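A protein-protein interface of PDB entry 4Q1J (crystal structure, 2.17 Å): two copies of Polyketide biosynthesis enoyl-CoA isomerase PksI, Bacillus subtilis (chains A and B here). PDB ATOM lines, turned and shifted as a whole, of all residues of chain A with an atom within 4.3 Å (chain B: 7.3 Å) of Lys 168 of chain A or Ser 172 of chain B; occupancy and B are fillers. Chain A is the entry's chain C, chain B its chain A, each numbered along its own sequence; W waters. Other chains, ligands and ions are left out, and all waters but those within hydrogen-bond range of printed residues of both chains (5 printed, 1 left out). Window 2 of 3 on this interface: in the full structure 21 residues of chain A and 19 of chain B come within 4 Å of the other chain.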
ATOM      1  N   LEU A 133      -7.455  19.557  13.451  1.00  0.00           N
ATOM      2  CA  LEU A 133      -7.231  20.645  14.331  1.00  0.00           C
ATOM      3  C   LEU A 133      -5.757  20.854  14.713  1.00  0.00           C
ATOM      4  O   LEU A 133      -5.467  21.927  15.198  1.00  0.00           O
ATOM      5  CB  LEU A 133      -8.086  20.586  15.583  1.00  0.00           C
ATOM      6  CG  LEU A 133      -9.555  20.869  15.401  1.00  0.00           C
ATOM      7  CD1 LEU A 133     -10.168  20.600  16.782  1.00  0.00           C
ATOM      8  CD2 LEU A 133      -9.912  22.275  14.943  1.00  0.00           C
ATOM      9  N   ALA A 135      -3.497  21.139  12.548  1.00  0.00           N
ATOM     10  CA  ALA A 135      -2.929  21.903  11.444  1.00  0.00           C
ATOM     11  C   ALA A 135      -2.619  23.283  11.986  1.00  0.00           C
ATOM     12  O   ALA A 135      -3.278  23.736  12.906  1.00  0.00           O
ATOM     13  CB  ALA A 135      -3.929  22.002  10.306  1.00  0.00           C
ATOM     14  N   ASP A 136      -1.663  23.970  11.369  1.00  0.00           N
ATOM     15  CA  ASP A 136      -1.332  25.337  11.758  1.00  0.00           C
ATOM     16  C   ASP A 136      -2.451  26.325  11.414  1.00  0.00           C
ATOM     17  O   ASP A 136      -2.614  27.342  12.089  1.00  0.00           O
ATOM     18  CB  ASP A 136      -0.023  25.777  11.098  1.00  0.00           C
ATOM     19  CG  ASP A 136       1.109  24.797  11.339  1.00  0.00           C
ATOM     20  OD1 ASP A 136       1.708  24.837  12.433  1.00  0.00           O
ATOM     21  OD2 ASP A 136       1.397  23.987  10.433  1.00  0.00           O
ATOM     22  N   ILE A 164      -5.819  19.723  22.085  1.00  0.00           N
ATOM     23  CA  ILE A 164      -5.901  20.612  20.869  1.00  0.00           C
ATOM     24  C   ILE A 164      -7.225  21.378  20.746  1.00  0.00           C
ATOM     25  O   ILE A 164      -7.245  22.417  20.123  1.00  0.00           O
ATOM     26  CB  ILE A 164      -5.581  19.815  19.587  1.00  0.00           C
ATOM     27  CG1 ILE A 164      -5.173  20.729  18.421  1.00  0.00           C
ATOM     28  CG2 ILE A 164      -6.674  18.788  19.235  1.00  0.00           C
ATOM     29  CD1 ILE A 164      -3.868  21.502  18.632  1.00  0.00           C
ATOM     30  N   VAL A 165      -8.328  20.879  21.325  1.00  0.00           N
ATOM     31  CA  VAL A 165      -9.601  21.609  21.239  1.00  0.00           C
ATOM     32  C   VAL A 165      -9.549  22.896  22.084  1.00  0.00           C
ATOM     33  O   VAL A 165      -9.819  23.985  21.547  1.00  0.00           O
ATOM     34  CB  VAL A 165     -10.880  20.747  21.530  1.00  0.00           C
ATOM     35  CG1 VAL A 165     -12.155  21.618  21.366  1.00  0.00           C
ATOM     36  CG2 VAL A 165     -10.957  19.558  20.563  1.00  0.00           C
ATOM     37  N   PRO A 166      -9.130  22.810  23.367  1.00  0.00           N
ATOM     38  CA  PRO A 166      -8.987  24.098  24.065  1.00  0.00           C
ATOM     39  C   PRO A 166      -7.859  24.988  23.509  1.00  0.00           C
ATOM     40  O   PRO A 166      -7.982  26.226  23.588  1.00  0.00           O
ATOM     41  CB  PRO A 166      -8.617  23.704  25.514  1.00  0.00           C
ATOM     42  CG  PRO A 166      -8.705  22.209  25.625  1.00  0.00           C
ATOM     43  CD  PRO A 166      -8.835  21.636  24.247  1.00  0.00           C
ATOM     44  N   LYS A 167      -6.752  24.398  23.045  1.00  0.00           N
ATOM     45  CA  LYS A 167      -5.656  25.179  22.527  1.00  0.00           C
ATOM     46  C   LYS A 167      -6.102  26.015  21.324  1.00  0.00           C
ATOM     47  O   LYS A 167      -5.698  27.150  21.208  1.00  0.00           O
ATOM     48  CB  LYS A 167      -4.557  24.267  22.001  1.00  0.00           C
ATOM     49  CG  LYS A 167      -3.263  25.066  21.704  1.00  0.00           C
ATOM     50  CD  LYS A 167      -2.664  25.408  23.071  1.00  0.00           C
ATOM     51  CE  LYS A 167      -1.473  26.346  23.005  1.00  0.00           C
ATOM     52  NZ  LYS A 167      -1.088  26.516  24.433  1.00  0.00           N
ATOM     53  N   LYS A 168      -6.890  25.427  20.411  1.00  0.00           N
ATOM     54  CA  LYS A 168      -7.325  26.149  19.192  1.00  0.00           C
ATOM     55  C   LYS A 168      -8.596  26.977  19.449  1.00  0.00           C
ATOM     56  O   LYS A 168      -8.656  28.120  19.017  1.00  0.00           O
ATOM     57  CB  LYS A 168      -7.501  25.214  17.970  1.00  0.00           C
ATOM     58  CG  LYS A 168      -6.206  24.513  17.513  1.00  0.00           C
ATOM     59  CD  LYS A 168      -5.213  25.505  16.840  1.00  0.00           C
ATOM     60  CE  LYS A 168      -4.309  24.909  15.693  1.00  0.00           C
ATOM     61  NZ  LYS A 168      -4.198  26.022  14.596  1.00  0.00           N
ATOM     62  N   LEU A 169      -9.616  26.383  20.126  1.00  0.00           N
ATOM     63  CA  LEU A 169     -10.911  27.009  20.275  1.00  0.00           C
ATOM     64  C   LEU A 169     -11.157  27.738  21.615  1.00  0.00           C
ATOM     65  O   LEU A 169     -12.205  28.373  21.800  1.00  0.00           O
ATOM     66  CB  LEU A 169     -12.015  25.947  19.999  1.00  0.00           C
ATOM     67  CG  LEU A 169     -11.978  25.473  18.533  1.00  0.00           C
ATOM     68  CD1 LEU A 169     -13.095  24.513  18.204  1.00  0.00           C
ATOM     69  CD2 LEU A 169     -12.031  26.628  17.551  1.00  0.00           C
ATOM     70  N   GLY A 170     -10.223  27.604  22.567  1.00  0.00           N
ATOM     71  CA  GLY A 170     -10.307  28.285  23.859  1.00  0.00           C
ATOM     72  C   GLY A 170     -10.928  27.341  24.867  1.00  0.00           C
ATOM     73  O   GLY A 170     -11.822  26.502  24.515  1.00  0.00           O
ATOM     74  N   PRO A 195     -11.812  31.369  15.945  1.00  0.00           N
ATOM     75  CA  PRO A 195     -10.795  32.159  15.216  1.00  0.00           C
ATOM     76  C   PRO A 195     -10.524  31.647  13.781  1.00  0.00           C
ATOM     77  O   PRO A 195      -9.851  32.328  13.029  1.00  0.00           O
ATOM     78  CB  PRO A 195      -9.567  32.036  16.118  1.00  0.00           C
ATOM     79  CG  PRO A 195      -9.728  30.684  16.774  1.00  0.00           C
ATOM     80  CD  PRO A 195     -11.222  30.734  17.150  1.00  0.00           C
ATOM     81  N   PHE A 196     -11.047  30.466  13.419  1.00  0.00           N
ATOM     82  CA  PHE A 196     -10.904  29.893  12.093  1.00  0.00           C
ATOM     83  C   PHE A 196     -11.691  30.691  11.030  1.00  0.00           C
ATOM     84  O   PHE A 196     -12.797  31.131  11.282  1.00  0.00           O
ATOM     85  CB  PHE A 196     -11.453  28.425  12.064  1.00  0.00           C
ATOM     86  CG  PHE A 196     -10.825  27.506  13.066  1.00  0.00           C
ATOM     87  CD1 PHE A 196      -9.569  27.787  13.603  1.00  0.00           C
ATOM     88  CD2 PHE A 196     -11.474  26.313  13.425  1.00  0.00           C
ATOM     89  CE1 PHE A 196      -8.996  26.939  14.514  1.00  0.00           C
ATOM     90  CE2 PHE A 196     -10.898  25.416  14.319  1.00  0.00           C
ATOM     91  CZ  PHE A 196      -9.656  25.733  14.883  1.00  0.00           C
ATOM     92  N   PRO B 166      -0.053  35.572  20.505  1.00  0.00           N
ATOM     93  CA  PRO B 166      -0.886  34.467  21.072  1.00  0.00           C
ATOM     94  C   PRO B 166      -1.579  34.759  22.409  1.00  0.00           C
ATOM     95  O   PRO B 166      -2.745  34.343  22.637  1.00  0.00           O
ATOM     96  CB  PRO B 166       0.133  33.338  21.297  1.00  0.00           C
ATOM     97  CG  PRO B 166       1.270  33.648  20.388  1.00  0.00           C
ATOM     98  CD  PRO B 166       1.358  35.148  20.349  1.00  0.00           C
ATOM     99  N   LEU B 169      -4.426  37.357  21.238  1.00  0.00           N
ATOM    100  CA  LEU B 169      -5.394  37.062  20.129  1.00  0.00           C
ATOM    101  C   LEU B 169      -5.683  35.607  20.100  1.00  0.00           C
ATOM    102  O   LEU B 169      -6.476  35.111  19.267  1.00  0.00           O
ATOM    103  CB  LEU B 169      -4.877  37.523  18.749  1.00  0.00           C
ATOM    104  CG  LEU B 169      -4.496  39.017  18.739  1.00  0.00           C
ATOM    105  CD1 LEU B 169      -4.239  39.444  17.328  1.00  0.00           C
ATOM    106  CD2 LEU B 169      -5.686  39.804  19.238  1.00  0.00           C
ATOM    107  N   GLY B 170      -5.083  34.886  21.022  1.00  0.00           N
ATOM    108  CA  GLY B 170      -5.284  33.449  21.015  1.00  0.00           C
ATOM    109  C   GLY B 170      -4.247  32.747  20.146  1.00  0.00           C
ATOM    110  O   GLY B 170      -3.713  33.283  19.154  1.00  0.00           O
ATOM    111  N   PHE B 171      -3.978  31.505  20.513  1.00  0.00           N
ATOM    112  CA  PHE B 171      -3.033  30.711  19.811  1.00  0.00           C
ATOM    113  C   PHE B 171      -3.267  30.642  18.291  1.00  0.00           C
ATOM    114  O   PHE B 171      -2.362  30.825  17.474  1.00  0.00           O
ATOM    115  CB  PHE B 171      -3.040  29.293  20.419  1.00  0.00           C
ATOM    116  CG  PHE B 171      -2.007  28.402  19.789  1.00  0.00           C
ATOM    117  CD1 PHE B 171      -0.652  28.594  20.061  1.00  0.00           C
ATOM    118  CD2 PHE B 171      -2.373  27.418  18.868  1.00  0.00           C
ATOM    119  CE1 PHE B 171       0.335  27.779  19.480  1.00  0.00           C
ATOM    120  CE2 PHE B 171      -1.392  26.603  18.284  1.00  0.00           C
ATOM    121  CZ  PHE B 171      -0.033  26.805  18.573  1.00  0.00           C
ATOM    122  N   SER B 172      -4.496  30.336  17.907  1.00  0.00           N
ATOM    123  CA  SER B 172      -4.746  29.959  16.553  1.00  0.00           C
ATOM    124  C   SER B 172      -4.573  31.091  15.569  1.00  0.00           C
ATOM    125  O   SER B 172      -3.984  30.897  14.491  1.00  0.00           O
ATOM    126  CB  SER B 172      -6.175  29.360  16.441  1.00  0.00           C
ATOM    127  OG  SER B 172      -6.535  29.380  15.097  1.00  0.00           O
ATOM    128  N   LEU B 173      -5.160  32.254  15.887  1.00  0.00           N
ATOM    129  CA  LEU B 173      -5.116  33.414  14.971  1.00  0.00           C
ATOM    130  C   LEU B 173      -3.623  33.962  14.953  1.00  0.00           C
ATOM    131  O   LEU B 173      -3.133  34.397  13.913  1.00  0.00           O
ATOM    132  CB  LEU B 173      -6.077  34.492  15.497  1.00  0.00           C
ATOM    133  CG  LEU B 173      -6.409  35.598  14.522  1.00  0.00           C
ATOM    134  CD1 LEU B 173      -6.987  35.091  13.195  1.00  0.00           C
ATOM    135  CD2 LEU B 173      -7.304  36.670  15.164  1.00  0.00           C
ATOM    136  N   ALA B 174      -2.939  33.889  16.110  1.00  0.00           N
ATOM    137  CA  ALA B 174      -1.483  34.058  16.187  1.00  0.00           C
ATOM    138  C   ALA B 174      -0.682  33.230  15.182  1.00  0.00           C
ATOM    139  O   ALA B 174       0.224  33.824  14.563  1.00  0.00           O
ATOM    140  CB  ALA B 174      -0.963  33.816  17.605  1.00  0.00           C
ATOM    141  N   GLN B 175      -0.980  31.924  14.984  1.00  0.00           N
ATOM    142  CA  GLN B 175      -0.260  31.104  13.986  1.00  0.00           C
ATOM    143  C   GLN B 175      -0.312  31.762  12.590  1.00  0.00           C
ATOM    144  O   GLN B 175       0.762  31.961  11.904  1.00  0.00           O
ATOM    145  CB  GLN B 175      -0.782  29.644  13.913  1.00  0.00           C
ATOM    146  CG  GLN B 175      -0.911  29.001  15.276  1.00  0.00           C
ATOM    147  CD  GLN B 175       0.372  29.185  16.041  1.00  0.00           C
ATOM    148  OE1 GLN B 175       1.392  28.646  15.627  1.00  0.00           O
ATOM    149  NE2 GLN B 175       0.360  30.008  17.105  1.00  0.00           N
ATOM    150  N   GLU B 176      -1.533  32.120  12.171  1.00  0.00           N
ATOM    151  CA  GLU B 176      -1.757  32.776  10.889  1.00  0.00           C
ATOM    152  C   GLU B 176      -1.065  34.176  10.806  1.00  0.00           C
ATOM    153  O   GLU B 176      -0.429  34.484   9.811  1.00  0.00           O
ATOM    154  CB  GLU B 176      -3.248  32.930  10.622  1.00  0.00           C
ATOM    155  CG  GLU B 176      -3.593  33.366   9.219  1.00  0.00           C
ATOM    156  CD  GLU B 176      -5.100  33.716   9.137  1.00  0.00           C
ATOM    157  OE1 GLU B 176      -5.884  32.805   9.429  1.00  0.00           O
ATOM    158  OE2 GLU B 176      -5.518  34.885   8.829  1.00  0.00           O
ATOM    159  N   ILE B 177      -1.269  35.013  11.807  1.00  0.00           N
ATOM    160  CA  ILE B 177      -0.730  36.344  11.796  1.00  0.00           C
ATOM    161  C   ILE B 177       0.805  36.307  11.682  1.00  0.00           C
ATOM    162  O   ILE B 177       1.399  37.059  10.907  1.00  0.00           O
ATOM    163  CB  ILE B 177      -1.157  37.113  13.073  1.00  0.00           C
ATOM    164  CG1 ILE B 177      -2.615  37.513  12.914  1.00  0.00           C
ATOM    165  CG2 ILE B 177      -0.206  38.365  13.425  1.00  0.00           C
ATOM    166  CD1 ILE B 177      -3.255  38.038  14.177  1.00  0.00           C
ATOM    167  N   ARG B 192     -12.958  38.361  12.560  1.00  0.00           N
ATOM    168  CA  ARG B 192     -12.266  37.147  12.976  1.00  0.00           C
ATOM    169  C   ARG B 192     -12.451  36.831  14.461  1.00  0.00           C
ATOM    170  O   ARG B 192     -11.968  35.806  14.943  1.00  0.00           O
ATOM    171  CB  ARG B 192     -10.775  37.244  12.644  1.00  0.00           C
ATOM    172  CG  ARG B 192     -10.459  37.112  11.164  1.00  0.00           C
ATOM    173  CD  ARG B 192     -10.708  35.697  10.669  1.00  0.00           C
ATOM    174  NE  ARG B 192      -9.776  35.316   9.611  1.00  0.00           N
ATOM    175  CZ  ARG B 192      -8.806  34.418   9.758  1.00  0.00           C
ATOM    176  NH1 ARG B 192      -8.638  33.805  10.921  1.00  0.00           N
ATOM    177  NH2 ARG B 192      -8.005  34.133   8.740  1.00  0.00           N
HETATM  178  O   HOH W   1       2.817  26.878  13.565  1.00  0.00           O
HETATM  179  O   HOH W   2      -7.131  31.202  13.429  1.00  0.00           O
HETATM  180  O   HOH W   3      -4.141  29.712  12.397  1.00  0.00           O
HETATM  181  O   HOH W   4      -6.774  30.068  19.672  1.00  0.00           O
HETATM  182  O   HOH W   5      -6.226  27.497  13.213  1.00  0.00           O
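NH1 of Arg 192 of chain B lies within hydrogen-bond range of O of Pro 195 of chain A (2.8 Å).
O of Asp 136 of chain A touches CB of Gln 175 of chain B (3.5 Å). Lys 167 of chain A touches Phe 171 of chain B. Phe 171 of chain B touches Lys 168 of chain A (CD2 to CD, 3.98 Å). Lys 168 of chain A touches Ser 172 of chain B (O to CB, 3.8 Å). CB of Ser 172 of chain B touches CG of Pro 195 of chain A, 3.8 Å away. Leu 173 of chain B touches Pro 195 of chain A. CE1 of Phe 196 of chain A touches OG of Ser 172 of chain B, 3.5 Å away.
Printed residues of chain B within 4 Å of Lys 168 of chain A: Phe 171 and Ser 172. Of chain A, only Lys 168 (3.8 Å), Pro 195 (3.8 Å) and Phe 196 (3.5 Å) come within 4 Å of Ser 172 of chain B. Of the printed residues of chain B, Phe 196 of chain A touches Ser 172. Printed residues of chain B within 4 Å of Lys 167 of chain A: Phe 171. Of the printed residues of chain A, Gln 175 of chain B touches Asp 136 (3.5 Å). Of the printed residues of chain A, Arg 192 of chain B touches Pro 195.
Water W3 bridges O of Ser 172 of chain B (2.4 Å) and O of Asp 136 of chain A (2.8 Å). Water W2 lies within hydrogen-bond range of the side-chain hydroxyl (OG) of Ser 172 of chain B (2.5 Å), the backbone carbonyl oxygen (O) of Pro 195 of chain A (3.0 Å) and the backbone NH (N) of Leu 173 of chain B (3.3 Å). Water W1 lies within hydrogen-bond range of the side-chain carboxylate (OD1) of Asp 136 of chain A and the side-chain amide oxygen (OE1) of Gln 175 of chain B. Water W5 bridges the side-chain hydroxyl of Ser 172 of chain B (2.7 Å) and the side-chain amino group of Lys 168 of chain A (2.9 Å). Water W4 lies within hydrogen-bond range of O of Lys 168 of chain A (2.8 Å), N of Ser 172 of chain B (2.9 Å), N of Phe 171 of chain B (3.3 Å) and O of Lys 167 of chain A (3.5 Å).
The backbone carbonyl oxygen (O) of Asp 136 of chain A lies within hydrogen-bond range of the side-chain amino group (NZ) of Lys 168 of chain A, at 3.2 Å. O of Ala 135 of chain A lies within hydrogen-bond range of NZ of Lys 168 of chain A (3.0 Å). The backbone carbonyl oxygen (O) of Phe 171 of chain B is in hydrogen-bond range of the side-chain amide nitrogen (NE2) of Gln 175 of chain B, at 2.9 Å. The side-chain carboxylate of Glu 176 of chain B is in salt-bridge range of the guanidinium group of Arg 192 of chain B.
Of the 11 printed residues of chain B, 5 touch a printed residue of chain A. Hydrophobic or aromatic side chains of chain B within 4 Å of the printed part of chain A: Phe 171 and Leu 173.
Positions printed for both chains: 166, 169 and 170.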
